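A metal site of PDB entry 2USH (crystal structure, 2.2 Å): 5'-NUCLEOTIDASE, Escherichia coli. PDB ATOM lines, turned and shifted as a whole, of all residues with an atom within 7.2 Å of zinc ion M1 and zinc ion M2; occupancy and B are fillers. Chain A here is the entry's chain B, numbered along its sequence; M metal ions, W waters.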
ATOM      1  N   ASN A  40      11.210 -20.119  -0.241  1.00  0.00           N
ATOM      2  CA  ASN A  40      10.595 -21.396  -0.554  1.00  0.00           C
ATOM      3  C   ASN A  40       9.262 -21.557   0.181  1.00  0.00           C
ATOM      4  O   ASN A  40       8.954 -20.807   1.114  1.00  0.00           O
ATOM      5  CB  ASN A  40      11.556 -22.541  -0.146  1.00  0.00           C
ATOM      6  CG  ASN A  40      11.957 -22.453   1.326  1.00  0.00           C
ATOM      7  OD1 ASN A  40      12.887 -21.702   1.694  1.00  0.00           O
ATOM      8  ND2 ASN A  40      11.268 -23.209   2.167  1.00  0.00           N
ATOM      9  N   ASP A  41       8.468 -22.512  -0.287  1.00  0.00           N
ATOM     10  CA  ASP A  41       7.185 -22.830   0.292  1.00  0.00           C
ATOM     11  C   ASP A  41       6.365 -21.586   0.621  1.00  0.00           C
ATOM     12  O   ASP A  41       5.894 -21.397   1.746  1.00  0.00           O
ATOM     13  CB  ASP A  41       7.442 -23.708   1.502  1.00  0.00           C
ATOM     14  CG  ASP A  41       8.177 -25.003   1.098  1.00  0.00           C
ATOM     15  OD1 ASP A  41       7.503 -25.973   0.708  1.00  0.00           O
ATOM     16  OD2 ASP A  41       9.421 -25.071   1.152  1.00  0.00           O
ATOM     17  N   HIS A  42       6.203 -20.753  -0.409  1.00  0.00           N
ATOM     18  CA  HIS A  42       5.444 -19.510  -0.377  1.00  0.00           C
ATOM     19  C   HIS A  42       4.003 -19.764   0.093  1.00  0.00           C
ATOM     20  O   HIS A  42       3.428 -18.990   0.867  1.00  0.00           O
ATOM     21  CB  HIS A  42       5.444 -18.920  -1.792  1.00  0.00           C
ATOM     22  CG  HIS A  42       4.618 -17.674  -1.921  1.00  0.00           C
ATOM     23  ND1 HIS A  42       4.988 -16.464  -1.377  1.00  0.00           N
ATOM     24  CD2 HIS A  42       3.440 -17.454  -2.555  1.00  0.00           C
ATOM     25  CE1 HIS A  42       4.087 -15.548  -1.677  1.00  0.00           C
ATOM     26  NE2 HIS A  42       3.134 -16.130  -2.395  1.00  0.00           N
ATOM     27  N   HIS A  43       3.416 -20.855  -0.393  1.00  0.00           N
ATOM     28  CA  HIS A  43       2.055 -21.243  -0.028  1.00  0.00           C
ATOM     29  C   HIS A  43       0.977 -20.160   0.054  1.00  0.00           C
ATOM     30  O   HIS A  43       0.320 -19.973   1.085  1.00  0.00           O
ATOM     31  CB  HIS A  43       2.105 -22.092   1.243  1.00  0.00           C
ATOM     32  CG  HIS A  43       2.692 -23.450   1.021  1.00  0.00           C
ATOM     33  ND1 HIS A  43       2.185 -24.326   0.082  1.00  0.00           N
ATOM     34  CD2 HIS A  43       3.730 -24.088   1.609  1.00  0.00           C
ATOM     35  CE1 HIS A  43       2.881 -25.449   0.108  1.00  0.00           C
ATOM     36  NE2 HIS A  43       3.822 -25.324   1.024  1.00  0.00           N
ATOM     37  N   GLY A  82      12.367 -22.338  -3.909  1.00  0.00           N
ATOM     38  CA  GLY A  82      12.380 -23.774  -3.665  1.00  0.00           C
ATOM     39  C   GLY A  82      11.042 -24.433  -3.965  1.00  0.00           C
ATOM     40  O   GLY A  82      10.861 -25.641  -3.724  1.00  0.00           O
ATOM     41  N   GLY A  83      10.072 -23.675  -4.468  1.00  0.00           N
ATOM     42  CA  GLY A  83       8.802 -24.288  -4.825  1.00  0.00           C
ATOM     43  C   GLY A  83       7.645 -24.190  -3.846  1.00  0.00           C
ATOM     44  O   GLY A  83       7.752 -23.547  -2.817  1.00  0.00           O
ATOM     45  N   ASP A  84       6.548 -24.871  -4.143  1.00  0.00           N
ATOM     46  CA  ASP A  84       5.341 -24.798  -3.330  1.00  0.00           C
ATOM     47  C   ASP A  84       4.775 -23.391  -3.223  1.00  0.00           C
ATOM     48  O   ASP A  84       4.686 -22.820  -2.128  1.00  0.00           O
ATOM     49  CB  ASP A  84       5.556 -25.421  -1.944  1.00  0.00           C
ATOM     50  CG  ASP A  84       5.267 -26.923  -1.934  1.00  0.00           C
ATOM     51  OD1 ASP A  84       4.894 -27.460  -3.000  1.00  0.00           O
ATOM     52  OD2 ASP A  84       5.363 -27.565  -0.856  1.00  0.00           O
ATOM     53  N   ILE A  85       4.361 -22.856  -4.379  1.00  0.00           N
ATOM     54  CA  ILE A  85       3.779 -21.515  -4.479  1.00  0.00           C
ATOM     55  C   ILE A  85       2.268 -21.662  -4.164  1.00  0.00           C
ATOM     56  O   ILE A  85       1.666 -20.815  -3.484  1.00  0.00           O
ATOM     57  CB  ILE A  85       3.981 -20.932  -5.939  1.00  0.00           C
ATOM     58  CG1 ILE A  85       5.468 -20.983  -6.303  1.00  0.00           C
ATOM     59  CG2 ILE A  85       3.446 -19.477  -6.038  1.00  0.00           C
ATOM     60  CD1 ILE A  85       6.368 -20.344  -5.274  1.00  0.00           C
ATOM     61  N   ASN A  86       1.713 -22.765  -4.634  1.00  0.00           N
ATOM     62  CA  ASN A  86       0.310 -23.114  -4.442  1.00  0.00           C
ATOM     63  C   ASN A  86      -0.078 -23.613  -3.057  1.00  0.00           C
ATOM     64  O   ASN A  86       0.731 -24.274  -2.384  1.00  0.00           O
ATOM     65  CB  ASN A  86      -0.098 -24.242  -5.408  1.00  0.00           C
ATOM     66  CG  ASN A  86      -0.118 -23.819  -6.876  1.00  0.00           C
ATOM     67  OD1 ASN A  86      -1.138 -23.357  -7.358  1.00  0.00           O
ATOM     68  ND2 ASN A  86       1.002 -24.007  -7.584  1.00  0.00           N
ATOM     69  N   THR A  87      -1.322 -23.315  -2.683  1.00  0.00           N
ATOM     70  CA  THR A  87      -1.991 -23.813  -1.466  1.00  0.00           C
ATOM     71  C   THR A  87      -1.602 -23.298  -0.090  1.00  0.00           C
ATOM     72  O   THR A  87      -0.499 -23.570   0.378  1.00  0.00           O
ATOM     73  CB  THR A  87      -1.852 -25.323  -1.400  1.00  0.00           C
ATOM     74  OG1 THR A  87      -2.223 -25.878  -2.657  1.00  0.00           O
ATOM     75  CG2 THR A  87      -2.769 -25.871  -0.381  1.00  0.00           C
ATOM     76  N   GLY A 115       7.295 -27.819  -6.623  1.00  0.00           N
ATOM     77  CA  GLY A 115       7.009 -28.448  -5.351  1.00  0.00           C
ATOM     78  C   GLY A 115       5.851 -29.418  -5.426  1.00  0.00           C
ATOM     79  O   GLY A 115       5.056 -29.360  -6.357  1.00  0.00           O
ATOM     80  N   ASN A 116       5.747 -30.288  -4.426  1.00  0.00           N
ATOM     81  CA  ASN A 116       4.662 -31.268  -4.389  1.00  0.00           C
ATOM     82  C   ASN A 116       3.293 -30.619  -4.461  1.00  0.00           C
ATOM     83  O   ASN A 116       2.427 -31.147  -5.144  1.00  0.00           O
ATOM     84  CB  ASN A 116       4.760 -32.176  -3.165  1.00  0.00           C
ATOM     85  CG  ASN A 116       4.693 -31.432  -1.845  1.00  0.00           C
ATOM     86  OD1 ASN A 116       5.313 -30.401  -1.663  1.00  0.00           O
ATOM     87  ND2 ASN A 116       3.959 -31.985  -0.893  1.00  0.00           N
ATOM     88  N   HIS A 117       3.091 -29.477  -3.807  1.00  0.00           N
ATOM     89  CA  HIS A 117       1.796 -28.827  -3.901  1.00  0.00           C
ATOM     90  C   HIS A 117       1.455 -28.171  -5.235  1.00  0.00           C
ATOM     91  O   HIS A 117       0.354 -27.668  -5.407  1.00  0.00           O
ATOM     92  CB  HIS A 117       1.597 -27.827  -2.752  1.00  0.00           C
ATOM     93  CG  HIS A 117       1.418 -28.499  -1.430  1.00  0.00           C
ATOM     94  ND1 HIS A 117       0.183 -28.930  -0.983  1.00  0.00           N
ATOM     95  CD2 HIS A 117       2.300 -28.832  -0.464  1.00  0.00           C
ATOM     96  CE1 HIS A 117       0.316 -29.509   0.193  1.00  0.00           C
ATOM     97  NE2 HIS A 117       1.599 -29.464   0.533  1.00  0.00           N
ATOM     98  N   THR A 172      10.581 -33.699  -4.776  1.00  0.00           N
ATOM     99  CA  THR A 172      10.467 -34.917  -3.947  1.00  0.00           C
ATOM    100  C   THR A 172       9.601 -36.034  -4.566  1.00  0.00           C
ATOM    101  O   THR A 172       8.580 -35.775  -5.225  1.00  0.00           O
ATOM    102  CB  THR A 172       9.890 -34.621  -2.513  1.00  0.00           C
ATOM    103  OG1 THR A 172       9.710 -35.852  -1.812  1.00  0.00           O
ATOM    104  CG2 THR A 172       8.559 -33.870  -2.573  1.00  0.00           C
ATOM    105  N   THR A 175       5.726 -36.936  -3.530  1.00  0.00           N
ATOM    106  CA  THR A 175       4.590 -36.218  -4.140  1.00  0.00           C
ATOM    107  C   THR A 175       3.434 -37.145  -4.545  1.00  0.00           C
ATOM    108  O   THR A 175       2.307 -36.980  -4.120  1.00  0.00           O
ATOM    109  CB  THR A 175       5.049 -35.405  -5.383  1.00  0.00           C
ATOM    110  OG1 THR A 175       6.072 -34.477  -4.995  1.00  0.00           O
ATOM    111  CG2 THR A 175       3.896 -34.608  -5.995  1.00  0.00           C
ATOM    112  N   HIS A 217      13.011 -29.362  -4.009  1.00  0.00           N
ATOM    113  CA  HIS A 217      11.857 -29.373  -3.138  1.00  0.00           C
ATOM    114  C   HIS A 217      11.885 -30.796  -2.559  1.00  0.00           C
ATOM    115  O   HIS A 217      11.091 -31.645  -2.939  1.00  0.00           O
ATOM    116  CB  HIS A 217      10.565 -29.134  -3.911  1.00  0.00           C
ATOM    117  CG  HIS A 217       9.421 -28.870  -3.012  1.00  0.00           C
ATOM    118  ND1 HIS A 217       9.206 -27.631  -2.444  1.00  0.00           N
ATOM    119  CD2 HIS A 217       8.537 -29.704  -2.420  1.00  0.00           C
ATOM    120  CE1 HIS A 217       8.251 -27.719  -1.537  1.00  0.00           C
ATOM    121  NE2 HIS A 217       7.832 -28.966  -1.505  1.00  0.00           N
ATOM    122  N   MET A 218      12.817 -31.019  -1.611  1.00  0.00           N
ATOM    123  CA  MET A 218      13.041 -32.315  -1.003  1.00  0.00           C
ATOM    124  C   MET A 218      13.078 -32.383   0.544  1.00  0.00           C
ATOM    125  O   MET A 218      12.718 -33.407   1.146  1.00  0.00           O
ATOM    126  CB  MET A 218      14.342 -32.837  -1.565  1.00  0.00           C
ATOM    127  CG  MET A 218      14.273 -32.924  -3.066  1.00  0.00           C
ATOM    128  SD  MET A 218      15.791 -33.406  -3.931  1.00  0.00           S
ATOM    129  CE  MET A 218      16.399 -34.673  -2.902  1.00  0.00           C
ATOM    130  N   GLY A 251      13.660 -26.726   0.119  1.00  0.00           N
ATOM    131  CA  GLY A 251      12.308 -26.422   0.539  1.00  0.00           C
ATOM    132  C   GLY A 251      11.604 -27.637   1.091  1.00  0.00           C
ATOM    133  O   GLY A 251      12.270 -28.579   1.537  1.00  0.00           O
ATOM    134  N   HIS A 252      10.272 -27.576   1.108  1.00  0.00           N
ATOM    135  CA  HIS A 252       9.417 -28.690   1.516  1.00  0.00           C
ATOM    136  C   HIS A 252       9.322 -29.021   2.998  1.00  0.00           C
ATOM    137  O   HIS A 252       8.227 -29.058   3.545  1.00  0.00           O
ATOM    138  CB  HIS A 252       9.835 -29.935   0.770  1.00  0.00           C
ATOM    139  CG  HIS A 252       8.894 -31.079   0.958  1.00  0.00           C
ATOM    140  ND1 HIS A 252       7.562 -30.990   0.616  1.00  0.00           N
ATOM    141  CD2 HIS A 252       9.082 -32.332   1.424  1.00  0.00           C
ATOM    142  CE1 HIS A 252       6.968 -32.147   0.859  1.00  0.00           C
ATOM    143  NE2 HIS A 252       7.871 -32.971   1.351  1.00  0.00           N
ATOM    144  N   SER A 253      10.439 -29.301   3.662  1.00  0.00           N
ATOM    145  CA  SER A 253      10.371 -29.593   5.092  1.00  0.00           C
ATOM    146  C   SER A 253       9.974 -28.280   5.781  1.00  0.00           C
ATOM    147  O   SER A 253       9.460 -28.259   6.881  1.00  0.00           O
ATOM    148  CB  SER A 253      11.723 -30.134   5.626  1.00  0.00           C
ATOM    149  OG  SER A 253      12.819 -29.255   5.390  1.00  0.00           O
ATOM    150  N   GLN A 254      10.266 -27.153   5.127  1.00  0.00           N
ATOM    151  CA  GLN A 254       9.924 -25.825   5.638  1.00  0.00           C
ATOM    152  C   GLN A 254      10.559 -25.407   6.925  1.00  0.00           C
ATOM    153  O   GLN A 254       9.869 -25.142   7.901  1.00  0.00           O
ATOM    154  CB  GLN A 254       8.407 -25.698   5.724  1.00  0.00           C
ATOM    155  CG  GLN A 254       7.781 -25.845   4.374  1.00  0.00           C
ATOM    156  CD  GLN A 254       6.322 -25.625   4.385  1.00  0.00           C
ATOM    157  OE1 GLN A 254       5.598 -26.175   3.570  1.00  0.00           O
ATOM    158  NE2 GLN A 254       5.866 -24.797   5.290  1.00  0.00           N
ATOM    159  N   HIS A 289      12.797 -21.380   5.431  1.00  0.00           N
ATOM    160  CA  HIS A 289      11.605 -21.648   6.218  1.00  0.00           C
ATOM    161  C   HIS A 289      10.315 -21.734   5.416  1.00  0.00           C
ATOM    162  O   HIS A 289      10.045 -22.767   4.821  1.00  0.00           O
ATOM    163  CB  HIS A 289      11.499 -20.576   7.309  1.00  0.00           C
ATOM    164  CG  HIS A 289      10.521 -20.920   8.397  1.00  0.00           C
ATOM    165  ND1 HIS A 289      10.049 -22.193   8.599  1.00  0.00           N
ATOM    166  CD2 HIS A 289       9.950 -20.150   9.345  1.00  0.00           C
ATOM    167  CE1 HIS A 289       9.209 -22.199   9.621  1.00  0.00           C
ATOM    168  NE2 HIS A 289       9.138 -20.965  10.097  1.00  0.00           N
ATOM    169  N   GLU A 290       9.539 -20.653   5.354  1.00  0.00           N
ATOM    170  CA  GLU A 290       8.253 -20.704   4.639  1.00  0.00           C
ATOM    171  C   GLU A 290       7.557 -19.363   4.555  1.00  0.00           C
ATOM    172  O   GLU A 290       7.911 -18.424   5.233  1.00  0.00           O
ATOM    173  CB  GLU A 290       7.307 -21.608   5.395  1.00  0.00           C
ATOM    174  CG  GLU A 290       7.055 -21.036   6.785  1.00  0.00           C
ATOM    175  CD  GLU A 290       6.214 -21.911   7.652  1.00  0.00           C
ATOM    176  OE1 GLU A 290       6.042 -23.090   7.322  1.00  0.00           O
ATOM    177  OE2 GLU A 290       5.728 -21.422   8.677  1.00  0.00           O
ATOM    178  N   TRP A 291       6.548 -19.298   3.688  1.00  0.00           N
ATOM    179  CA  TRP A 291       5.677 -18.124   3.552  1.00  0.00           C
ATOM    180  C   TRP A 291       6.236 -16.743   3.266  1.00  0.00           C
ATOM    181  O   TRP A 291       5.502 -15.764   3.425  1.00  0.00           O
ATOM    182  CB  TRP A 291       4.817 -18.005   4.809  1.00  0.00           C
ATOM    183  CG  TRP A 291       4.017 -19.228   5.106  1.00  0.00           C
ATOM    184  CD1 TRP A 291       3.939 -20.375   4.377  1.00  0.00           C
ATOM    185  CD2 TRP A 291       3.194 -19.417   6.255  1.00  0.00           C
ATOM    186  NE1 TRP A 291       3.099 -21.279   4.994  1.00  0.00           N
ATOM    187  CE2 TRP A 291       2.634 -20.713   6.154  1.00  0.00           C
ATOM    188  CE3 TRP A 291       2.858 -18.616   7.361  1.00  0.00           C
ATOM    189  CZ2 TRP A 291       1.766 -21.227   7.125  1.00  0.00           C
ATOM    190  CZ3 TRP A 291       1.992 -19.133   8.312  1.00  0.00           C
ATOM    191  CH2 TRP A 291       1.452 -20.417   8.192  1.00  0.00           C
ATOM    192  N   THR A 518       0.631 -32.835   5.934  1.00  0.00           N
ATOM    193  CA  THR A 518       0.119 -32.744   4.568  1.00  0.00           C
ATOM    194  C   THR A 518       0.236 -31.385   3.914  1.00  0.00           C
ATOM    195  O   THR A 518       0.165 -31.272   2.712  1.00  0.00           O
ATOM    196  CB  THR A 518      -1.371 -33.134   4.479  1.00  0.00           C
ATOM    197  OG1 THR A 518      -2.151 -32.129   5.148  1.00  0.00           O
ATOM    198  CG2 THR A 518      -1.618 -34.516   5.151  1.00  0.00           C
ATOM    199  N   GLY A 519       0.400 -30.334   4.706  1.00  0.00           N
ATOM    200  CA  GLY A 519       0.484 -29.028   4.085  1.00  0.00           C
ATOM    201  C   GLY A 519      -0.901 -28.480   3.780  1.00  0.00           C
ATOM    202  O   GLY A 519      -1.029 -27.352   3.297  1.00  0.00           O
HETATM  203 ZN    ZN M   1       5.488 -26.662   1.393  1.00  0.00          ZN
HETATM  204 ZN    ZN M   2       6.416 -29.378  -0.210  1.00  0.00          ZN
HETATM  205  O   HOH W   1       6.106 -28.455   1.189  1.00  0.00           O
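The backbone NH (N) of Thr 172 sits at hydrogen-bond distance from the backbone carbonyl oxygen (O) of His 217 (2.8 Å).
N of His 252 is in hydrogen-bond range of OD2 of Asp 41, at 2.6 Å.
O of Thr 87 is in hydrogen-bond range of ND1 of His 43 (2.8 Å).
OD1 of Asp 84 lies within hydrogen-bond range of N of His 117, 2.8 Å away.
O of Asp 84 is in hydrogen-bond range of N of His 42, at 3.1 Å.
ND1 of His 289 lies within hydrogen-bond range of O of Gln 254 (3.0 Å).
The backbone NH of Asp 41 sits at hydrogen-bond distance from the backbone carbonyl oxygen of Gly 83 (2.8 Å).
O of Asp 41 is in hydrogen-bond range of N of Trp 291 (2.9 Å).
Water W1 is bound to zinc ion M2 (1.7 Å).
NE2 of His 217 is bound to zinc ion M2 (2.0 Å).
The side-chain amide oxygen (OD1) of Asn 116 is bound to zinc ion M2 (2.1 Å).
A ring nitrogen (ND1) of His 252 binds zinc ion M2, 2.1 Å away.
OD2 of Asp 84 binds zinc ion M2.
Zinc ion M2 has five donor atoms within binding distance.
The nearest printed residue that does not touch zinc ion M1 is His 217 (4.2 Å).
Five residues have an atom within 4 Å of zinc ion M2: Asp 41, Asp 84, Asn 116, His 217 and His 252.
The nearest printed residue that does not touch zinc ion M2 is His 117 (4.2 Å).
Zinc ion M1 is bound by water W1 (1.9 Å), NE2 of His 43 (2.2 Å), OE1 of Gln 254 (2.2 Å), OD1 of Asp 41 (2.2 Å) and OD2 of Asp 84 (2.4 Å).
Zinc ion M1 has five donor atoms within binding distance.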
